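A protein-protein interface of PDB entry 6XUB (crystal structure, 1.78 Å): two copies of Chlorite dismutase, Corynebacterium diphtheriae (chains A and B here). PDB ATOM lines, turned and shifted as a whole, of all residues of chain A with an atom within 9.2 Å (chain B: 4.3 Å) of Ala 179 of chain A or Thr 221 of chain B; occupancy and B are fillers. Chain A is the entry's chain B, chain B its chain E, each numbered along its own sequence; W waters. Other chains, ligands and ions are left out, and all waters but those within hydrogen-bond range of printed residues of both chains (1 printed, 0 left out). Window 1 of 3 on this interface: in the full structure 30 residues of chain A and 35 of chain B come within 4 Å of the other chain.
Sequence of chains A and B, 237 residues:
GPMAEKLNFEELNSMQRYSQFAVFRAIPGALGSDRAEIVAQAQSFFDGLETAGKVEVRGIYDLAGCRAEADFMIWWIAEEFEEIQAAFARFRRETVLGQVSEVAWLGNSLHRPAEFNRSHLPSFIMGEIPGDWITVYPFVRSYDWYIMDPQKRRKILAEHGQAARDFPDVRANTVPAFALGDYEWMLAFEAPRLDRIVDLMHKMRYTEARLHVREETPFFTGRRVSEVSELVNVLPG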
ATOM      1  N   TYR A  18     -25.780 -17.016  27.004  1.00  0.00           N
ATOM      2  CA  TYR A  18     -24.422 -16.565  27.262  1.00  0.00           C
ATOM      3  C   TYR A  18     -24.424 -15.488  28.337  1.00  0.00           C
ATOM      4  O   TYR A  18     -25.402 -14.762  28.519  1.00  0.00           O
ATOM      5  CB  TYR A  18     -23.789 -16.004  26.002  1.00  0.00           C
ATOM      6  CG  TYR A  18     -23.516 -17.044  24.966  1.00  0.00           C
ATOM      7  CD1 TYR A  18     -24.504 -17.446  24.078  1.00  0.00           C
ATOM      8  CD2 TYR A  18     -22.259 -17.659  24.881  1.00  0.00           C
ATOM      9  CE1 TYR A  18     -24.251 -18.406  23.110  1.00  0.00           C
ATOM     10  CE2 TYR A  18     -21.987 -18.614  23.918  1.00  0.00           C
ATOM     11  CZ  TYR A  18     -22.992 -19.003  23.034  1.00  0.00           C
ATOM     12  OH  TYR A  18     -22.751 -19.969  22.055  1.00  0.00           O
ATOM     13  N   PHE A  81     -24.306 -15.122  21.516  1.00  0.00           N
ATOM     14  CA  PHE A  81     -23.082 -14.410  21.866  1.00  0.00           C
ATOM     15  C   PHE A  81     -22.897 -13.189  20.981  1.00  0.00           C
ATOM     16  O   PHE A  81     -22.387 -12.165  21.443  1.00  0.00           O
ATOM     17  CB  PHE A  81     -21.846 -15.327  21.781  1.00  0.00           C
ATOM     18  CG  PHE A  81     -20.622 -14.713  22.394  1.00  0.00           C
ATOM     19  CD1 PHE A  81     -20.555 -14.511  23.769  1.00  0.00           C
ATOM     20  CD2 PHE A  81     -19.554 -14.315  21.606  1.00  0.00           C
ATOM     21  CE1 PHE A  81     -19.439 -13.908  24.357  1.00  0.00           C
ATOM     22  CE2 PHE A  81     -18.427 -13.737  22.187  1.00  0.00           C
ATOM     23  CZ  PHE A  81     -18.380 -13.528  23.571  1.00  0.00           C
ATOM     24  N   GLN A  85     -21.594  -9.392  21.840  1.00  0.00           N
ATOM     25  CA  GLN A  85     -20.499  -8.809  21.074  1.00  0.00           C
ATOM     26  C   GLN A  85     -20.873  -7.429  20.571  1.00  0.00           C
ATOM     27  O   GLN A  85     -20.088  -6.468  20.677  1.00  0.00           O
ATOM     28  CB  GLN A  85     -20.151  -9.696  19.882  1.00  0.00           C
ATOM     29  CG  GLN A  85     -19.389 -10.914  20.159  1.00  0.00           C
ATOM     30  CD  GLN A  85     -18.817 -11.473  18.872  1.00  0.00           C
ATOM     31  OE1 GLN A  85     -19.556 -11.884  17.991  1.00  0.00           O
ATOM     32  NE2 GLN A  85     -17.496 -11.446  18.743  1.00  0.00           N
ATOM     33  N   LEU A 106     -12.254  -9.753  30.285  1.00  0.00           N
ATOM     34  CA  LEU A 106     -13.558 -10.290  29.899  1.00  0.00           C
ATOM     35  C   LEU A 106     -13.669 -11.742  30.343  1.00  0.00           C
ATOM     36  O   LEU A 106     -12.783 -12.540  30.057  1.00  0.00           O
ATOM     37  CB  LEU A 106     -13.757 -10.190  28.371  1.00  0.00           C
ATOM     38  CG  LEU A 106     -13.692  -8.765  27.838  1.00  0.00           C
ATOM     39  CD1 LEU A 106     -13.600  -8.688  26.354  1.00  0.00           C
ATOM     40  CD2 LEU A 106     -14.949  -7.987  28.301  1.00  0.00           C
ATOM     41  N   ASN A 108     -16.289 -14.820  29.794  1.00  0.00           N
ATOM     42  CA  ASN A 108     -17.423 -15.280  28.998  1.00  0.00           C
ATOM     43  C   ASN A 108     -17.795 -16.685  29.429  1.00  0.00           C
ATOM     44  O   ASN A 108     -16.944 -17.484  29.835  1.00  0.00           O
ATOM     45  CB  ASN A 108     -17.077 -15.258  27.501  1.00  0.00           C
ATOM     46  CG  ASN A 108     -16.728 -13.868  27.022  1.00  0.00           C
ATOM     47  OD1 ASN A 108     -17.503 -12.937  27.224  1.00  0.00           O
ATOM     48  ND2 ASN A 108     -15.559 -13.705  26.452  1.00  0.00           N
ATOM     49  N   SER A 109     -19.074 -16.994  29.300  1.00  0.00           N
ATOM     50  CA  SER A 109     -19.550 -18.316  29.667  1.00  0.00           C
ATOM     51  C   SER A 109     -20.883 -18.608  28.987  1.00  0.00           C
ATOM     52  O   SER A 109     -21.550 -17.716  28.477  1.00  0.00           O
ATOM     53  CB  SER A 109     -19.713 -18.441  31.177  1.00  0.00           C
ATOM     54  OG  SER A 109     -20.565 -17.447  31.679  1.00  0.00           O
ATOM     55  N   LEU A 110     -21.270 -19.878  29.056  1.00  0.00           N
ATOM     56  CA  LEU A 110     -22.458 -20.402  28.393  1.00  0.00           C
ATOM     57  C   LEU A 110     -23.072 -21.420  29.337  1.00  0.00           C
ATOM     58  O   LEU A 110     -22.430 -22.419  29.664  1.00  0.00           O
ATOM     59  CB  LEU A 110     -22.101 -21.062  27.060  1.00  0.00           C
ATOM     60  CG  LEU A 110     -23.258 -21.823  26.368  1.00  0.00           C
ATOM     61  CD1 LEU A 110     -24.443 -20.854  26.074  1.00  0.00           C
ATOM     62  CD2 LEU A 110     -22.743 -22.519  25.112  1.00  0.00           C
ATOM     63  N   PRO A 176     -20.006 -22.922  32.413  1.00  0.00           N
ATOM     64  CA  PRO A 176     -18.943 -23.310  31.491  1.00  0.00           C
ATOM     65  C   PRO A 176     -18.411 -22.145  30.703  1.00  0.00           C
ATOM     66  O   PRO A 176     -19.156 -21.316  30.175  1.00  0.00           O
ATOM     67  CB  PRO A 176     -19.623 -24.330  30.564  1.00  0.00           C
ATOM     68  CG  PRO A 176     -20.660 -24.902  31.364  1.00  0.00           C
ATOM     69  CD  PRO A 176     -21.161 -23.817  32.295  1.00  0.00           C
ATOM     70  N   ALA A 177     -17.093 -22.132  30.568  1.00  0.00           N
ATOM     71  CA  ALA A 177     -16.412 -21.085  29.825  1.00  0.00           C
ATOM     72  C   ALA A 177     -15.488 -21.660  28.749  1.00  0.00           C
ATOM     73  O   ALA A 177     -14.763 -20.893  28.100  1.00  0.00           O
ATOM     74  CB  ALA A 177     -15.620 -20.203  30.816  1.00  0.00           C
ATOM     75  N   PHE A 178     -15.508 -22.978  28.541  1.00  0.00           N
ATOM     76  CA  PHE A 178     -14.640 -23.618  27.556  1.00  0.00           C
ATOM     77  C   PHE A 178     -14.736 -22.919  26.207  1.00  0.00           C
ATOM     78  O   PHE A 178     -15.832 -22.709  25.671  1.00  0.00           O
ATOM     79  CB  PHE A 178     -15.022 -25.100  27.363  1.00  0.00           C
ATOM     80  CG  PHE A 178     -15.088 -25.889  28.638  1.00  0.00           C
ATOM     81  CD1 PHE A 178     -13.955 -26.464  29.183  1.00  0.00           C
ATOM     82  CD2 PHE A 178     -16.284 -26.061  29.293  1.00  0.00           C
ATOM     83  CE1 PHE A 178     -14.026 -27.169  30.359  1.00  0.00           C
ATOM     84  CE2 PHE A 178     -16.357 -26.778  30.461  1.00  0.00           C
ATOM     85  CZ  PHE A 178     -15.225 -27.300  31.017  1.00  0.00           C
ATOM     86  N   ALA A 179     -13.589 -22.586  25.651  1.00  0.00           N
ATOM     87  CA  ALA A 179     -13.450 -22.023  24.313  1.00  0.00           C
ATOM     88  C   ALA A 179     -13.987 -20.602  24.187  1.00  0.00           C
ATOM     89  O   ALA A 179     -14.006 -20.058  23.080  1.00  0.00           O
ATOM     90  CB  ALA A 179     -14.122 -22.909  23.255  1.00  0.00           C
ATOM     91  N   LEU A 180     -14.385 -19.960  25.281  1.00  0.00           N
ATOM     92  CA  LEU A 180     -14.787 -18.550  25.247  1.00  0.00           C
ATOM     93  C   LEU A 180     -13.714 -17.633  25.834  1.00  0.00           C
ATOM     94  O   LEU A 180     -14.004 -16.506  26.258  1.00  0.00           O
ATOM     95  CB  LEU A 180     -16.123 -18.387  25.974  1.00  0.00           C
ATOM     96  CG  LEU A 180     -17.201 -19.362  25.506  1.00  0.00           C
ATOM     97  CD1 LEU A 180     -18.418 -19.296  26.397  1.00  0.00           C
ATOM     98  CD2 LEU A 180     -17.548 -19.032  24.064  1.00  0.00           C
ATOM     99  N   GLY A 181     -12.482 -18.111  25.887  1.00  0.00           N
ATOM    100  CA  GLY A 181     -11.420 -17.434  26.590  1.00  0.00           C
ATOM    101  C   GLY A 181     -10.446 -18.478  27.093  1.00  0.00           C
ATOM    102  O   GLY A 181     -10.449 -19.598  26.613  1.00  0.00           O
ATOM    103  N   ASP A 182      -9.664 -18.104  28.103  1.00  0.00           N
ATOM    104  CA  ASP A 182      -8.580 -18.968  28.575  1.00  0.00           C
ATOM    105  C   ASP A 182      -9.016 -19.981  29.632  1.00  0.00           C
ATOM    106  O   ASP A 182      -8.153 -20.699  30.168  1.00  0.00           O
ATOM    107  CB  ASP A 182      -7.450 -18.113  29.142  1.00  0.00           C
ATOM    108  CG  ASP A 182      -6.690 -17.403  28.072  1.00  0.00           C
ATOM    109  OD1 ASP A 182      -6.919 -17.701  26.877  1.00  0.00           O
ATOM    110  OD2 ASP A 182      -5.878 -16.528  28.408  1.00  0.00           O
ATOM    111  N   TYR A 183     -10.318 -20.075  29.938  1.00  0.00           N
ATOM    112  CA  TYR A 183     -10.738 -20.780  31.136  1.00  0.00           C
ATOM    113  C   TYR A 183     -11.730 -21.901  30.869  1.00  0.00           C
ATOM    114  O   TYR A 183     -12.210 -22.115  29.752  1.00  0.00           O
ATOM    115  CB  TYR A 183     -11.289 -19.778  32.158  1.00  0.00           C
ATOM    116  CG  TYR A 183     -10.467 -18.539  32.245  1.00  0.00           C
ATOM    117  CD1 TYR A 183      -9.225 -18.540  32.873  1.00  0.00           C
ATOM    118  CD2 TYR A 183     -10.928 -17.352  31.710  1.00  0.00           C
ATOM    119  CE1 TYR A 183      -8.467 -17.392  32.955  1.00  0.00           C
ATOM    120  CE2 TYR A 183     -10.175 -16.196  31.790  1.00  0.00           C
ATOM    121  CZ  TYR A 183      -8.946 -16.224  32.413  1.00  0.00           C
ATOM    122  OH  TYR A 183      -8.209 -15.065  32.489  1.00  0.00           O
ATOM    123  N   GLU A 184     -11.993 -22.655  31.930  1.00  0.00           N
ATOM    124  CA  GLU A 184     -12.959 -23.736  31.902  1.00  0.00           C
ATOM    125  C   GLU A 184     -14.312 -23.369  32.488  1.00  0.00           C
ATOM    126  O   GLU A 184     -15.337 -23.827  31.968  1.00  0.00           O
ATOM    127  CB  GLU A 184     -12.403 -24.928  32.670  1.00  0.00           C
ATOM    128  CG  GLU A 184     -11.201 -25.511  31.965  1.00  0.00           C
ATOM    129  CD  GLU A 184     -10.617 -26.724  32.647  1.00  0.00           C
ATOM    130  OE1 GLU A 184     -11.066 -27.106  33.753  1.00  0.00           O
ATOM    131  OE2 GLU A 184      -9.677 -27.286  32.039  1.00  0.00           O
ATOM    132  N   TRP A 185     -14.325 -22.608  33.596  1.00  0.00           N
ATOM    133  CA  TRP A 185     -15.538 -22.123  34.220  1.00  0.00           C
ATOM    134  C   TRP A 185     -15.439 -20.632  34.519  1.00  0.00           C
ATOM    135  O   TRP A 185     -14.365 -20.085  34.763  1.00  0.00           O
ATOM    136  CB  TRP A 185     -15.823 -22.902  35.532  1.00  0.00           C
ATOM    137  CG  TRP A 185     -15.906 -24.399  35.269  1.00  0.00           C
ATOM    138  CD1 TRP A 185     -14.858 -25.292  35.206  1.00  0.00           C
ATOM    139  CD2 TRP A 185     -17.095 -25.145  35.008  1.00  0.00           C
ATOM    140  NE1 TRP A 185     -15.345 -26.563  34.916  1.00  0.00           N
ATOM    141  CE2 TRP A 185     -16.710 -26.486  34.781  1.00  0.00           C
ATOM    142  CE3 TRP A 185     -18.468 -24.801  34.916  1.00  0.00           C
ATOM    143  CZ2 TRP A 185     -17.645 -27.493  34.499  1.00  0.00           C
ATOM    144  CZ3 TRP A 185     -19.392 -25.824  34.623  1.00  0.00           C
ATOM    145  CH2 TRP A 185     -18.965 -27.144  34.416  1.00  0.00           C
ATOM    146  N   LEU B  63     -13.306 -10.449  16.853  1.00  0.00           N
ATOM    147  CA  LEU B  63     -13.059 -11.003  18.179  1.00  0.00           C
ATOM    148  C   LEU B  63     -13.674 -10.159  19.299  1.00  0.00           C
ATOM    149  O   LEU B  63     -13.390 -10.408  20.480  1.00  0.00           O
ATOM    150  CB  LEU B  63     -11.550 -11.157  18.433  1.00  0.00           C
ATOM    151  CG  LEU B  63     -10.783 -11.975  17.385  1.00  0.00           C
ATOM    152  CD1 LEU B  63      -9.354 -12.147  17.925  1.00  0.00           C
ATOM    153  CD2 LEU B  63     -11.378 -13.299  17.121  1.00  0.00           C
ATOM    154  N   CYS B  66     -14.162 -11.191  23.151  1.00  0.00           N
ATOM    155  CA  CYS B  66     -13.569 -12.463  23.549  1.00  0.00           C
ATOM    156  C   CYS B  66     -12.605 -12.258  24.707  1.00  0.00           C
ATOM    157  O   CYS B  66     -12.696 -12.950  25.737  1.00  0.00           O
ATOM    158  CB  CYS B  66     -12.870 -13.122  22.370  1.00  0.00           C
ATOM    159  SG  CYS B  66     -11.734 -14.476  22.903  1.00  0.00           S
ATOM    160  N   ILE B 134     -15.218 -19.481  15.015  1.00  0.00           N
ATOM    161  CA  ILE B 134     -13.909 -20.101  15.131  1.00  0.00           C
ATOM    162  C   ILE B 134     -13.356 -19.908  16.542  1.00  0.00           C
ATOM    163  O   ILE B 134     -13.583 -18.890  17.201  1.00  0.00           O
ATOM    164  CB  ILE B 134     -12.936 -19.521  14.067  1.00  0.00           C
ATOM    165  CG1 ILE B 134     -11.788 -20.480  13.810  1.00  0.00           C
ATOM    166  CG2 ILE B 134     -12.395 -18.174  14.520  1.00  0.00           C
ATOM    167  CD1 ILE B 134     -10.927 -20.078  12.593  1.00  0.00           C
ATOM    168  N   THR B 135     -12.624 -20.921  17.012  1.00  0.00           N
ATOM    169  CA  THR B 135     -11.776 -20.789  18.182  1.00  0.00           C
ATOM    170  C   THR B 135     -10.383 -21.279  17.785  1.00  0.00           C
ATOM    171  O   THR B 135     -10.235 -22.355  17.193  1.00  0.00           O
ATOM    172  CB  THR B 135     -12.324 -21.549  19.403  1.00  0.00           C
ATOM    173  OG1 THR B 135     -11.630 -21.099  20.583  1.00  0.00           O
ATOM    174  CG2 THR B 135     -12.138 -23.027  19.268  1.00  0.00           C
ATOM    175  N   LEU B 194     -21.502 -21.148  17.818  1.00  0.00           N
ATOM    176  CA  LEU B 194     -20.446 -21.087  18.832  1.00  0.00           C
ATOM    177  C   LEU B 194     -20.664 -22.140  19.913  1.00  0.00           C
ATOM    178  O   LEU B 194     -19.706 -22.671  20.474  1.00  0.00           O
ATOM    179  CB  LEU B 194     -20.408 -19.693  19.445  1.00  0.00           C
ATOM    180  CG  LEU B 194     -19.398 -19.439  20.573  1.00  0.00           C
ATOM    181  CD1 LEU B 194     -18.002 -19.841  20.150  1.00  0.00           C
ATOM    182  CD2 LEU B 194     -19.456 -17.944  21.021  1.00  0.00           C
ATOM    183  N   ILE B 197     -18.872 -25.397  19.508  1.00  0.00           N
ATOM    184  CA  ILE B 197     -17.457 -25.371  19.895  1.00  0.00           C
ATOM    185  C   ILE B 197     -17.312 -25.483  21.409  1.00  0.00           C
ATOM    186  O   ILE B 197     -16.472 -26.246  21.911  1.00  0.00           O
ATOM    187  CB  ILE B 197     -16.750 -24.110  19.364  1.00  0.00           C
ATOM    188  CG1 ILE B 197     -16.766 -24.031  17.834  1.00  0.00           C
ATOM    189  CG2 ILE B 197     -15.311 -24.117  19.810  1.00  0.00           C
ATOM    190  CD1 ILE B 197     -16.411 -22.635  17.281  1.00  0.00           C
ATOM    191  N   MET B 201     -15.298 -28.757  23.101  1.00  0.00           N
ATOM    192  CA  MET B 201     -14.199 -28.562  24.047  1.00  0.00           C
ATOM    193  C   MET B 201     -14.499 -29.221  25.389  1.00  0.00           C
ATOM    194  O   MET B 201     -13.631 -29.884  25.968  1.00  0.00           O
ATOM    195  CB  MET B 201     -13.938 -27.061  24.224  1.00  0.00           C
ATOM    196  CG  MET B 201     -12.595 -26.716  24.851  1.00  0.00           C
ATOM    197  SD  MET B 201     -11.206 -27.277  23.848  1.00  0.00           S
ATOM    198  CE  MET B 201     -11.641 -26.586  22.244  1.00  0.00           C
ATOM    199  N   PHE B 219      -6.477 -18.304  23.941  1.00  0.00           N
ATOM    200  CA  PHE B 219      -7.631 -18.570  23.090  1.00  0.00           C
ATOM    201  C   PHE B 219      -8.111 -17.302  22.398  1.00  0.00           C
ATOM    202  O   PHE B 219      -8.233 -16.237  23.023  1.00  0.00           O
ATOM    203  CB  PHE B 219      -8.786 -19.114  23.946  1.00  0.00           C
ATOM    204  CG  PHE B 219      -8.847 -20.593  24.017  1.00  0.00           C
ATOM    205  CD1 PHE B 219      -8.014 -21.281  24.902  1.00  0.00           C
ATOM    206  CD2 PHE B 219      -9.780 -21.299  23.272  1.00  0.00           C
ATOM    207  CE1 PHE B 219      -8.065 -22.672  24.965  1.00  0.00           C
ATOM    208  CE2 PHE B 219      -9.856 -22.673  23.353  1.00  0.00           C
ATOM    209  CZ  PHE B 219      -8.984 -23.355  24.202  1.00  0.00           C
ATOM    210  N   PHE B 220      -8.459 -17.446  21.128  1.00  0.00           N
ATOM    211  CA  PHE B 220      -9.106 -16.385  20.351  1.00  0.00           C
ATOM    212  C   PHE B 220     -10.361 -16.977  19.723  1.00  0.00           C
ATOM    213  O   PHE B 220     -10.295 -17.952  18.959  1.00  0.00           O
ATOM    214  CB  PHE B 220      -8.153 -15.796  19.295  1.00  0.00           C
ATOM    215  CG  PHE B 220      -6.843 -15.343  19.888  1.00  0.00           C
ATOM    216  CD1 PHE B 220      -6.697 -14.079  20.445  1.00  0.00           C
ATOM    217  CD2 PHE B 220      -5.783 -16.218  19.962  1.00  0.00           C
ATOM    218  CE1 PHE B 220      -5.496 -13.704  21.034  1.00  0.00           C
ATOM    219  CE2 PHE B 220      -4.564 -15.833  20.570  1.00  0.00           C
ATOM    220  CZ  PHE B 220      -4.412 -14.592  21.059  1.00  0.00           C
ATOM    221  N   THR B 221     -11.510 -16.421  20.090  1.00  0.00           N
ATOM    222  CA  THR B 221     -12.802 -16.905  19.633  1.00  0.00           C
ATOM    223  C   THR B 221     -13.539 -15.758  18.964  1.00  0.00           C
ATOM    224  O   THR B 221     -13.553 -14.641  19.490  1.00  0.00           O
ATOM    225  CB  THR B 221     -13.601 -17.446  20.810  1.00  0.00           C
ATOM    226  OG1 THR B 221     -12.921 -18.567  21.375  1.00  0.00           O
ATOM    227  CG2 THR B 221     -14.923 -17.913  20.359  1.00  0.00           C
ATOM    228  N   GLY B 222     -14.126 -16.013  17.795  1.00  0.00           N
ATOM    229  CA  GLY B 222     -14.783 -14.913  17.112  1.00  0.00           C
ATOM    230  C   GLY B 222     -15.591 -15.357  15.913  1.00  0.00           C
ATOM    231  O   GLY B 222     -15.644 -16.542  15.572  1.00  0.00           O
HETATM  232  O   HOH W   1     -11.369 -13.471  28.112  1.00  0.00           O
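No position is printed for both chains.
Of the 13 pairs that touch across the chains among the printed residues, none has its exchanged pair printed and touching as well.
Tyr 18 of chain A touches Leu 194 of chain B.
CB of Phe 81 of chain A touches CD2 of Leu 194 of chain B, 3.6 Å away.
Leu 106 of chain A touches Cys 66 of chain B (CB to O, 3.96 Å).
CB of Phe 178 of chain A touches CG of Met 201 of chain B, at 3.8 Å.
O of Ala 179 of chain A touches OG1 of Thr 135 of chain B, at 3.6 Å.
CG2 of Ile 197 of chain B touches CB of Ala 179 of chain A, at 3.8 Å.
Ala 179 of chain A touches Phe 219 of chain B.
O of Leu 180 of chain A touches O of Cys 66 of chain B, 3.8 Å away.
CD2 of Leu 180 of chain A touches CD2 of Leu 194 of chain B (3.8 Å).
Gly 181 of chain A touches Phe 219 of chain B (O to CB, 3.2 Å).
The backbone carbonyl oxygen of Leu 180 of chain A sits at hydrogen-bond distance from the side-chain amide nitrogen of Asn 108 of chain A, at 3.2 Å.
The side-chain sulfur (SG) of Cys 66 of chain B is in hydrogen-bond range of the backbone NH (N) of Thr 221 of chain B, 3.4 Å away.
The side-chain hydroxyl of Thr 135 of chain B lies within hydrogen-bond range of the side-chain hydroxyl of Thr 221 of chain B (3.0 Å).
Water W1 lies within hydrogen-bond range of the backbone carbonyl oxygen of Leu 106 of chain A (2.6 Å) and the backbone carbonyl oxygen of Cys 66 of chain B (2.8 Å).
Of the printed residues of chain B, Ala 179 of chain A touches Thr 135 (3.6 Å), Ile 197 (3.8 Å), Phe 219 (3.8 Å) and Thr 221 (2.5 Å).
Thr 221 of chain B touches just one residue of chain A: Ala 179.
No residue of chain A comes within 4 Å of Leu 63 of chain B.
No residue of chain A comes within 4 Å of Gly 222 of chain B.
Of the printed residues of chain B, Asp 182 of chain A touches Phe 219.
Printed residues of chain A within 4 Å of Ile 197 of chain B: Ala 179.
The nearest printed residue of chain B that does not touch Ala 179 of chain A is Met 201 of chain B (4.3 Å).
Hydrophobic or aromatic side chains of chain B within 4 Å of the printed part of chain A: Leu 194, Ile 197, Met 201 and Phe 219.
Of the 17 printed residues of chain A, 9 touch a printed residue of chain B.
Hydrophobic or aromatic side chains of chain A within 4 Å of the printed part of chain B: Tyr 18, Phe 81, Leu 106, Phe 178, Ala 179 and Leu 180.
Among the printed residues, 13 pairs touch across the chains.
The backbone carbonyl oxygen (O) of Cys 66 of chain B sits at hydrogen-bond distance from the side-chain amide nitrogen (ND2) of Asn 108 of chain A.
OD1 of Asp 182 of chain A lies within hydrogen-bond range of N of Phe 219 of chain B.
The backbone carbonyl oxygen (O) of Ala 179 of chain A is in hydrogen-bond range of the side-chain hydroxyl (OG1) of Thr 221 of chain B (2.5 Å).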
